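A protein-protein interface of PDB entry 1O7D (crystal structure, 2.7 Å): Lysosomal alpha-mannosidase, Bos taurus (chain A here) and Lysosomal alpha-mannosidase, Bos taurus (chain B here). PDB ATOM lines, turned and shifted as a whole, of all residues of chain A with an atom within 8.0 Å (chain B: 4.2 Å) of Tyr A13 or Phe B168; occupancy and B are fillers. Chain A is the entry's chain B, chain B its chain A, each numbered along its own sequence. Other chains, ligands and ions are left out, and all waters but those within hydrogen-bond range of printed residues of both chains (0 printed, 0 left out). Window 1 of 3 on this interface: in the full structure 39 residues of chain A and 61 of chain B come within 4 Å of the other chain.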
ATOM      1  N   TYR A   7       5.730  36.084 -33.574  1.00  0.00           N
ATOM      2  CA  TYR A   7       6.019  36.876 -32.379  1.00  0.00           C
ATOM      3  C   TYR A   7       6.135  35.847 -31.264  1.00  0.00           C
ATOM      4  O   TYR A   7       5.484  34.804 -31.308  1.00  0.00           O
ATOM      5  CB  TYR A   7       4.868  37.831 -32.047  1.00  0.00           C
ATOM      6  CG  TYR A   7       4.901  39.147 -32.788  1.00  0.00           C
ATOM      7  CD1 TYR A   7       5.991  40.008 -32.665  1.00  0.00           C
ATOM      8  CD2 TYR A   7       3.846  39.530 -33.621  1.00  0.00           C
ATOM      9  CE1 TYR A   7       6.029  41.221 -33.361  1.00  0.00           C
ATOM     10  CE2 TYR A   7       3.873  40.739 -34.323  1.00  0.00           C
ATOM     11  CZ  TYR A   7       4.965  41.578 -34.191  1.00  0.00           C
ATOM     12  OH  TYR A   7       5.010  42.762 -34.890  1.00  0.00           O
ATOM     13  N   SER A   8       6.941  36.124 -30.252  1.00  0.00           N
ATOM     14  CA  SER A   8       7.085  35.135 -29.199  1.00  0.00           C
ATOM     15  C   SER A   8       7.912  35.659 -28.041  1.00  0.00           C
ATOM     16  O   SER A   8       8.587  36.679 -28.157  1.00  0.00           O
ATOM     17  CB  SER A   8       7.727  33.866 -29.786  1.00  0.00           C
ATOM     18  OG  SER A   8       7.795  32.805 -28.850  1.00  0.00           O
ATOM     19  N   THR A   9       7.848  34.952 -26.923  1.00  0.00           N
ATOM     20  CA  THR A   9       8.595  35.330 -25.740  1.00  0.00           C
ATOM     21  C   THR A   9       9.579  34.211 -25.420  1.00  0.00           C
ATOM     22  O   THR A   9       9.407  33.070 -25.867  1.00  0.00           O
ATOM     23  CB  THR A   9       7.655  35.541 -24.525  1.00  0.00           C
ATOM     24  OG1 THR A   9       6.891  34.349 -24.311  1.00  0.00           O
ATOM     25  CG2 THR A   9       6.710  36.730 -24.754  1.00  0.00           C
ATOM     26  N   PRO A  10      10.640  34.525 -24.654  1.00  0.00           N
ATOM     27  CA  PRO A  10      11.637  33.520 -24.292  1.00  0.00           C
ATOM     28  C   PRO A  10      11.013  32.322 -23.608  1.00  0.00           C
ATOM     29  O   PRO A  10      11.557  31.223 -23.670  1.00  0.00           O
ATOM     30  CB  PRO A  10      12.573  34.290 -23.369  1.00  0.00           C
ATOM     31  CG  PRO A  10      12.565  35.642 -23.982  1.00  0.00           C
ATOM     32  CD  PRO A  10      11.086  35.862 -24.227  1.00  0.00           C
ATOM     33  N   ALA A  11       9.861  32.540 -22.971  1.00  0.00           N
ATOM     34  CA  ALA A  11       9.167  31.474 -22.252  1.00  0.00           C
ATOM     35  C   ALA A  11       8.448  30.509 -23.170  1.00  0.00           C
ATOM     36  O   ALA A  11       8.420  29.303 -22.913  1.00  0.00           O
ATOM     37  CB  ALA A  11       8.182  32.060 -21.256  1.00  0.00           C
ATOM     38  N   CYS A  12       7.867  31.035 -24.241  1.00  0.00           N
ATOM     39  CA  CYS A  12       7.150  30.182 -25.182  1.00  0.00           C
ATOM     40  C   CYS A  12       8.120  29.355 -26.007  1.00  0.00           C
ATOM     41  O   CYS A  12       7.836  28.219 -26.366  1.00  0.00           O
ATOM     42  CB  CYS A  12       6.246  31.029 -26.079  1.00  0.00           C
ATOM     43  SG  CYS A  12       4.844  31.703 -25.124  1.00  0.00           S
ATOM     44  N   TYR A  13       9.278  29.932 -26.289  1.00  0.00           N
ATOM     45  CA  TYR A  13      10.298  29.231 -27.044  1.00  0.00           C
ATOM     46  C   TYR A  13      10.811  28.080 -26.180  1.00  0.00           C
ATOM     47  O   TYR A  13      11.237  27.034 -26.681  1.00  0.00           O
ATOM     48  CB  TYR A  13      11.445  30.189 -27.390  1.00  0.00           C
ATOM     49  CG  TYR A  13      12.706  29.492 -27.818  1.00  0.00           C
ATOM     50  CD1 TYR A  13      12.725  28.692 -28.960  1.00  0.00           C
ATOM     51  CD2 TYR A  13      13.873  29.600 -27.067  1.00  0.00           C
ATOM     52  CE1 TYR A  13      13.881  28.005 -29.353  1.00  0.00           C
ATOM     53  CE2 TYR A  13      15.035  28.919 -27.440  1.00  0.00           C
ATOM     54  CZ  TYR A  13      15.033  28.123 -28.592  1.00  0.00           C
ATOM     55  OH  TYR A  13      16.182  27.461 -29.002  1.00  0.00           O
ATOM     56  N   LEU A  14      10.753  28.270 -24.870  1.00  0.00           N
ATOM     57  CA  LEU A  14      11.234  27.241 -23.971  1.00  0.00           C
ATOM     58  C   LEU A  14      10.204  26.144 -23.848  1.00  0.00           C
ATOM     59  O   LEU A  14      10.560  24.971 -23.681  1.00  0.00           O
ATOM     60  CB  LEU A  14      11.544  27.813 -22.582  1.00  0.00           C
ATOM     61  CG  LEU A  14      12.440  26.892 -21.738  1.00  0.00           C
ATOM     62  CD1 LEU A  14      13.853  26.890 -22.310  1.00  0.00           C
ATOM     63  CD2 LEU A  14      12.475  27.355 -20.315  1.00  0.00           C
ATOM     64  N   TRP A  15       8.927  26.515 -23.927  1.00  0.00           N
ATOM     65  CA  TRP A  15       7.884  25.511 -23.828  1.00  0.00           C
ATOM     66  C   TRP A  15       8.001  24.559 -25.002  1.00  0.00           C
ATOM     67  O   TRP A  15       7.821  23.357 -24.845  1.00  0.00           O
ATOM     68  CB  TRP A  15       6.502  26.163 -23.812  1.00  0.00           C
ATOM     69  CG  TRP A  15       5.368  25.181 -23.699  1.00  0.00           C
ATOM     70  CD1 TRP A  15       4.226  25.184 -24.437  1.00  0.00           C
ATOM     71  CD2 TRP A  15       5.276  24.037 -22.820  1.00  0.00           C
ATOM     72  NE1 TRP A  15       3.426  24.120 -24.085  1.00  0.00           N
ATOM     73  CE2 TRP A  15       4.045  23.400 -23.092  1.00  0.00           C
ATOM     74  CE3 TRP A  15       6.113  23.491 -21.833  1.00  0.00           C
ATOM     75  CZ2 TRP A  15       3.625  22.235 -22.420  1.00  0.00           C
ATOM     76  CZ3 TRP A  15       5.699  22.324 -21.162  1.00  0.00           C
ATOM     77  CH2 TRP A  15       4.464  21.714 -21.461  1.00  0.00           C
ATOM     78  N   GLU A  16       8.350  25.081 -26.170  1.00  0.00           N
ATOM     79  CA  GLU A  16       8.472  24.206 -27.336  1.00  0.00           C
ATOM     80  C   GLU A  16       9.656  23.275 -27.171  1.00  0.00           C
ATOM     81  O   GLU A  16       9.596  22.116 -27.561  1.00  0.00           O
ATOM     82  CB  GLU A  16       8.630  25.045 -28.610  1.00  0.00           C
ATOM     83  CG  GLU A  16       7.383  25.764 -29.049  1.00  0.00           C
ATOM     84  CD  GLU A  16       6.167  24.848 -29.129  1.00  0.00           C
ATOM     85  OE1 GLU A  16       6.262  23.728 -29.692  1.00  0.00           O
ATOM     86  OE2 GLU A  16       5.100  25.265 -28.633  1.00  0.00           O
ATOM     87  N   LEU A  17      10.737  23.775 -26.581  1.00  0.00           N
ATOM     88  CA  LEU A  17      11.930  22.945 -26.401  1.00  0.00           C
ATOM     89  C   LEU A  17      11.629  21.803 -25.453  1.00  0.00           C
ATOM     90  O   LEU A  17      12.148  20.697 -25.592  1.00  0.00           O
ATOM     91  CB  LEU A  17      13.099  23.783 -25.862  1.00  0.00           C
ATOM     92  CG  LEU A  17      13.462  25.027 -26.687  1.00  0.00           C
ATOM     93  CD1 LEU A  17      14.697  25.704 -26.060  1.00  0.00           C
ATOM     94  CD2 LEU A  17      13.730  24.641 -28.141  1.00  0.00           C
ATOM     95  N   ASN A  18      10.774  22.071 -24.479  1.00  0.00           N
ATOM     96  CA  ASN A  18      10.413  21.029 -23.536  1.00  0.00           C
ATOM     97  C   ASN A  18       9.559  19.989 -24.269  1.00  0.00           C
ATOM     98  O   ASN A  18       9.863  18.801 -24.244  1.00  0.00           O
ATOM     99  CB  ASN A  18       9.649  21.643 -22.356  1.00  0.00           C
ATOM    100  CG  ASN A  18       9.540  20.699 -21.175  1.00  0.00           C
ATOM    101  OD1 ASN A  18       8.501  20.089 -20.955  1.00  0.00           O
ATOM    102  ND2 ASN A  18      10.617  20.572 -20.413  1.00  0.00           N
ATOM    103  N   LYS A  19       8.513  20.463 -24.945  1.00  0.00           N
ATOM    104  CA  LYS A  19       7.574  19.615 -25.692  1.00  0.00           C
ATOM    105  C   LYS A  19       8.251  18.601 -26.587  1.00  0.00           C
ATOM    106  O   LYS A  19       7.674  17.564 -26.893  1.00  0.00           O
ATOM    107  CB  LYS A  19       6.643  20.458 -26.573  1.00  0.00           C
ATOM    108  CG  LYS A  19       5.843  21.507 -25.825  1.00  0.00           C
ATOM    109  CD  LYS A  19       5.003  22.353 -26.778  1.00  0.00           C
ATOM    110  CE  LYS A  19       3.735  21.615 -27.181  1.00  0.00           C
ATOM    111  NZ  LYS A  19       2.849  21.404 -25.967  1.00  0.00           N
ATOM    112  N   TRP A  24      19.325  16.313 -23.180  1.00  0.00           N
ATOM    113  CA  TRP A  24      20.398  17.275 -23.299  1.00  0.00           C
ATOM    114  C   TRP A  24      21.640  16.922 -22.499  1.00  0.00           C
ATOM    115  O   TRP A  24      21.564  16.217 -21.491  1.00  0.00           O
ATOM    116  CB  TRP A  24      19.879  18.648 -22.895  1.00  0.00           C
ATOM    117  CG  TRP A  24      19.020  19.282 -23.961  1.00  0.00           C
ATOM    118  CD1 TRP A  24      19.436  20.098 -25.003  1.00  0.00           C
ATOM    119  CD2 TRP A  24      17.603  19.186 -24.075  1.00  0.00           C
ATOM    120  NE1 TRP A  24      18.352  20.518 -25.743  1.00  0.00           N
ATOM    121  CE2 TRP A  24      17.214  19.975 -25.199  1.00  0.00           C
ATOM    122  CE3 TRP A  24      16.616  18.515 -23.337  1.00  0.00           C
ATOM    123  CZ2 TRP A  24      15.881  20.109 -25.590  1.00  0.00           C
ATOM    124  CZ3 TRP A  24      15.290  18.647 -23.726  1.00  0.00           C
ATOM    125  CH2 TRP A  24      14.934  19.438 -24.843  1.00  0.00           C
ATOM    126  N   HIS B  17      11.125  32.281 -33.570  1.00  0.00           N
ATOM    127  CA  HIS B  17      10.438  33.050 -32.529  1.00  0.00           C
ATOM    128  C   HIS B  17      11.019  34.448 -32.448  1.00  0.00           C
ATOM    129  O   HIS B  17      12.141  34.629 -31.963  1.00  0.00           O
ATOM    130  CB  HIS B  17      10.645  32.392 -31.173  1.00  0.00           C
ATOM    131  CG  HIS B  17       9.971  31.073 -31.032  1.00  0.00           C
ATOM    132  ND1 HIS B  17       8.659  30.948 -30.634  1.00  0.00           N
ATOM    133  CD2 HIS B  17      10.422  29.816 -31.236  1.00  0.00           C
ATOM    134  CE1 HIS B  17       8.334  29.671 -30.598  1.00  0.00           C
ATOM    135  NE2 HIS B  17       9.388  28.961 -30.959  1.00  0.00           N
ATOM    136  N   VAL B 142      11.332  32.294 -17.093  1.00  0.00           N
ATOM    137  CA  VAL B 142      12.735  32.128 -17.492  1.00  0.00           C
ATOM    138  C   VAL B 142      13.591  33.279 -16.962  1.00  0.00           C
ATOM    139  O   VAL B 142      13.064  34.330 -16.639  1.00  0.00           O
ATOM    140  CB  VAL B 142      12.867  32.095 -19.024  1.00  0.00           C
ATOM    141  CG1 VAL B 142      12.324  30.797 -19.557  1.00  0.00           C
ATOM    142  CG2 VAL B 142      12.105  33.249 -19.635  1.00  0.00           C
ATOM    143  N   ALA B 143      14.900  33.087 -16.856  1.00  0.00           N
ATOM    144  CA  ALA B 143      15.769  34.159 -16.373  1.00  0.00           C
ATOM    145  C   ALA B 143      16.462  34.775 -17.594  1.00  0.00           C
ATOM    146  O   ALA B 143      16.843  34.050 -18.523  1.00  0.00           O
ATOM    147  CB  ALA B 143      16.775  33.612 -15.382  1.00  0.00           C
ATOM    148  N   TRP B 144      16.664  36.091 -17.583  1.00  0.00           N
ATOM    149  CA  TRP B 144      17.206  36.780 -18.750  1.00  0.00           C
ATOM    150  C   TRP B 144      18.525  37.570 -18.663  1.00  0.00           C
ATOM    151  O   TRP B 144      18.516  38.789 -18.801  1.00  0.00           O
ATOM    152  CB  TRP B 144      16.085  37.690 -19.258  1.00  0.00           C
ATOM    153  CG  TRP B 144      16.276  38.377 -20.572  1.00  0.00           C
ATOM    154  CD1 TRP B 144      16.493  39.711 -20.770  1.00  0.00           C
ATOM    155  CD2 TRP B 144      16.160  37.797 -21.875  1.00  0.00           C
ATOM    156  NE1 TRP B 144      16.517  39.999 -22.113  1.00  0.00           N
ATOM    157  CE2 TRP B 144      16.322  38.839 -22.816  1.00  0.00           C
ATOM    158  CE3 TRP B 144      15.950  36.495 -22.345  1.00  0.00           C
ATOM    159  CZ2 TRP B 144      16.262  38.621 -24.195  1.00  0.00           C
ATOM    160  CZ3 TRP B 144      15.893  36.282 -23.726  1.00  0.00           C
ATOM    161  CH2 TRP B 144      16.055  37.339 -24.627  1.00  0.00           C
ATOM    162  N   HIS B 145      19.657  36.898 -18.461  1.00  0.00           N
ATOM    163  CA  HIS B 145      20.949  37.605 -18.404  1.00  0.00           C
ATOM    164  C   HIS B 145      21.591  37.694 -19.773  1.00  0.00           C
ATOM    165  O   HIS B 145      22.287  36.778 -20.216  1.00  0.00           O
ATOM    166  CB  HIS B 145      21.929  36.894 -17.492  1.00  0.00           C
ATOM    167  CG  HIS B 145      21.654  37.104 -16.045  1.00  0.00           C
ATOM    168  ND1 HIS B 145      22.595  36.857 -15.074  1.00  0.00           N
ATOM    169  CD2 HIS B 145      20.546  37.544 -15.408  1.00  0.00           C
ATOM    170  CE1 HIS B 145      22.078  37.137 -13.889  1.00  0.00           C
ATOM    171  NE2 HIS B 145      20.838  37.555 -14.063  1.00  0.00           N
ATOM    172  N   PHE B 167      16.970  29.655 -18.536  1.00  0.00           N
ATOM    173  CA  PHE B 167      17.899  30.777 -18.409  1.00  0.00           C
ATOM    174  C   PHE B 167      18.655  30.939 -19.745  1.00  0.00           C
ATOM    175  O   PHE B 167      19.294  29.993 -20.226  1.00  0.00           O
ATOM    176  CB  PHE B 167      18.858  30.452 -17.263  1.00  0.00           C
ATOM    177  CG  PHE B 167      20.015  31.386 -17.124  1.00  0.00           C
ATOM    178  CD1 PHE B 167      19.831  32.705 -16.729  1.00  0.00           C
ATOM    179  CD2 PHE B 167      21.308  30.910 -17.277  1.00  0.00           C
ATOM    180  CE1 PHE B 167      20.928  33.536 -16.470  1.00  0.00           C
ATOM    181  CE2 PHE B 167      22.408  31.722 -17.025  1.00  0.00           C
ATOM    182  CZ  PHE B 167      22.222  33.037 -16.619  1.00  0.00           C
ATOM    183  N   PHE B 168      18.556  32.125 -20.350  1.00  0.00           N
ATOM    184  CA  PHE B 168      19.221  32.415 -21.627  1.00  0.00           C
ATOM    185  C   PHE B 168      20.266  33.499 -21.448  1.00  0.00           C
ATOM    186  O   PHE B 168      20.089  34.381 -20.620  1.00  0.00           O
ATOM    187  CB  PHE B 168      18.219  32.932 -22.658  1.00  0.00           C
ATOM    188  CG  PHE B 168      16.989  32.091 -22.792  1.00  0.00           C
ATOM    189  CD1 PHE B 168      16.020  32.097 -21.791  1.00  0.00           C
ATOM    190  CD2 PHE B 168      16.791  31.293 -23.927  1.00  0.00           C
ATOM    191  CE1 PHE B 168      14.870  31.324 -21.910  1.00  0.00           C
ATOM    192  CE2 PHE B 168      15.653  30.519 -24.061  1.00  0.00           C
ATOM    193  CZ  PHE B 168      14.684  30.530 -23.050  1.00  0.00           C
ATOM    194  N   PHE B 169      21.342  33.455 -22.223  1.00  0.00           N
ATOM    195  CA  PHE B 169      22.347  34.501 -22.110  1.00  0.00           C
ATOM    196  C   PHE B 169      23.144  34.758 -23.379  1.00  0.00           C
ATOM    197  O   PHE B 169      23.202  33.915 -24.277  1.00  0.00           O
ATOM    198  CB  PHE B 169      23.293  34.223 -20.936  1.00  0.00           C
ATOM    199  CG  PHE B 169      24.086  32.966 -21.066  1.00  0.00           C
ATOM    200  CD1 PHE B 169      25.062  32.831 -22.049  1.00  0.00           C
ATOM    201  CD2 PHE B 169      23.883  31.917 -20.179  1.00  0.00           C
ATOM    202  CE1 PHE B 169      25.827  31.659 -22.146  1.00  0.00           C
ATOM    203  CE2 PHE B 169      24.640  30.744 -20.267  1.00  0.00           C
ATOM    204  CZ  PHE B 169      25.614  30.614 -21.250  1.00  0.00           C
ATOM    205  N   GLU B 187      22.535  24.549 -26.572  1.00  0.00           N
ATOM    206  CA  GLU B 187      21.607  24.419 -25.460  1.00  0.00           C
ATOM    207  C   GLU B 187      21.813  23.118 -24.722  1.00  0.00           C
ATOM    208  O   GLU B 187      22.037  22.064 -25.348  1.00  0.00           O
ATOM    209  CB  GLU B 187      20.173  24.480 -25.976  1.00  0.00           C
ATOM    210  CG  GLU B 187      20.086  25.031 -27.384  1.00  0.00           C
ATOM    211  CD  GLU B 187      18.667  25.086 -27.909  1.00  0.00           C
ATOM    212  OE1 GLU B 187      17.875  25.933 -27.425  1.00  0.00           O
ATOM    213  OE2 GLU B 187      18.353  24.272 -28.808  1.00  0.00           O
ATOM    214  N   SER B 206      20.290  28.287 -22.491  1.00  0.00           N
ATOM    215  CA  SER B 206      20.339  28.472 -23.926  1.00  0.00           C
ATOM    216  C   SER B 206      21.187  29.649 -24.367  1.00  0.00           C
ATOM    217  O   SER B 206      20.931  30.789 -23.977  1.00  0.00           O
ATOM    218  CB  SER B 206      18.932  28.656 -24.462  1.00  0.00           C
ATOM    219  OG  SER B 206      18.958  28.890 -25.852  1.00  0.00           O
ATOM    220  N   TYR B 258      20.979  24.850 -33.968  1.00  0.00           N
ATOM    221  CA  TYR B 258      20.196  24.363 -32.829  1.00  0.00           C
ATOM    222  C   TYR B 258      19.471  23.036 -33.065  1.00  0.00           C
ATOM    223  O   TYR B 258      19.016  22.742 -34.169  1.00  0.00           O
ATOM    224  CB  TYR B 258      19.190  25.428 -32.397  1.00  0.00           C
ATOM    225  CG  TYR B 258      19.827  26.689 -31.882  1.00  0.00           C
ATOM    226  CD1 TYR B 258      20.309  27.658 -32.759  1.00  0.00           C
ATOM    227  CD2 TYR B 258      19.933  26.921 -30.514  1.00  0.00           C
ATOM    228  CE1 TYR B 258      20.874  28.833 -32.285  1.00  0.00           C
ATOM    229  CE2 TYR B 258      20.493  28.088 -30.028  1.00  0.00           C
ATOM    230  CZ  TYR B 258      20.962  29.042 -30.916  1.00  0.00           C
ATOM    231  OH  TYR B 258      21.503  30.209 -30.424  1.00  0.00           O
ATOM    232  N   HIS B 262      13.168  24.815 -33.624  1.00  0.00           N
ATOM    233  CA  HIS B 262      12.967  26.154 -33.057  1.00  0.00           C
ATOM    234  C   HIS B 262      14.215  26.975 -32.778  1.00  0.00           C
ATOM    235  O   HIS B 262      15.221  26.452 -32.298  1.00  0.00           O
ATOM    236  CB  HIS B 262      12.212  26.044 -31.752  1.00  0.00           C
ATOM    237  CG  HIS B 262      10.820  25.506 -31.918  1.00  0.00           C
ATOM    238  ND1 HIS B 262       9.772  26.285 -32.351  1.00  0.00           N
ATOM    239  CD2 HIS B 262      10.332  24.270 -31.706  1.00  0.00           C
ATOM    240  CE1 HIS B 262       8.677  25.539 -32.388  1.00  0.00           C
ATOM    241  NE2 HIS B 262       8.984  24.321 -32.005  1.00  0.00           N
ATOM    242  N   THR B 263      14.131  28.276 -33.065  1.00  0.00           N
ATOM    243  CA  THR B 263      15.234  29.209 -32.804  1.00  0.00           C
ATOM    244  C   THR B 263      14.710  30.603 -32.496  1.00  0.00           C
ATOM    245  O   THR B 263      13.688  31.036 -33.024  1.00  0.00           O
ATOM    246  CB  THR B 263      16.216  29.359 -33.985  1.00  0.00           C
ATOM    247  OG1 THR B 263      16.205  28.176 -34.786  1.00  0.00           O
ATOM    248  CG2 THR B 263      17.639  29.581 -33.452  1.00  0.00           C
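A ring nitrogen (ND1) of His B17 is in hydrogen-bond range of the side-chain hydroxyl of Ser A8, 2.7 Å away. The side-chain carboxylate (OE1) of Glu B187 is in hydrogen-bond range of the side-chain hydroxyl (OH) of Tyr A13, 2.8 Å away.
A ring nitrogen (NE2) of His B17 is in hydrogen-bond range of a ring nitrogen (ND1) of His B262 (3.0 Å). The backbone carbonyl oxygen of Thr B263 is in hydrogen-bond range of the backbone NH of His B17, at 2.9 Å. The backbone carbonyl oxygen of Ala B143 lies within hydrogen-bond range of the backbone NH of Phe B168 (3.2 Å). The backbone NH (N) of His B145 is in hydrogen-bond range of the backbone carbonyl oxygen (O) of Phe B168, at 3.3 Å.
Among the printed residues, pairs that only touch across the chains: Pro A10 with Phe B168 (3.3 Å), Trp A24 with Glu B187 (3.3 Å), Pro A10 with Trp B144 (3.4 Å), Tyr A13 with His B17 (3.4 Å), Leu A17 with Glu B187 (3.5 Å), Glu A16 with His B262 (3.5 Å), Tyr A13 with His B262 (3.5 Å), Leu A14 with Val B142 (3.5 Å), Tyr A13 with Phe B168 (3.6 Å), Tyr A13 with Thr B263 (3.7 Å), Leu A14 with Phe B168 (3.8 Å) and Pro A10 with Val B142 (3.9 Å).
Of chain B, only His B17 (3.4 Å), Phe B168 (3.6 Å), Glu B187 (2.8 Å), His B262 (3.5 Å) and Thr B263 (3.7 Å) come within 4 Å of Tyr A13. Of the printed residues of chain B, Leu A14 touches Val B142 (3.5 Å) and Phe B168 (3.8 Å). Of the printed residues of chain A, His B17 touches Ser A8 and Tyr A13. Phe B167 touches none of the printed residues of chain A. Of chain A, only Pro A10 (3.3 Å), Tyr A13 (3.6 Å) and Leu A14 (3.8 Å) come within 4 Å of Phe B168. The nearest residue of chain A that does not touch Phe B168 is Ala A11 (5.2 Å). The nearest printed residue of chain B that does not touch Ser A8 is Thr B263 (7.4 Å).
Of the 13 printed residues of chain B, 7 touch a printed residue of chain A. Printed residues of chain B that touch a printed residue of chain A: His B17, Val B142, Trp B144, Phe B168, Glu B187, His B262 and Thr B263. Hydrophobic or aromatic side chains of chain B within 4 Å of the printed part of chain A: His B17, Val B142, Trp B144, Phe B168 and His B262. Of the 14 printed residues of chain A, 7 touch a printed residue of chain B. Among the printed residues, 14 pairs touch across the chains. Among the printed residues, no Asp or Glu carboxylate lies within 4 Å of a Lys or Arg side-chain nitrogen of the other chain.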
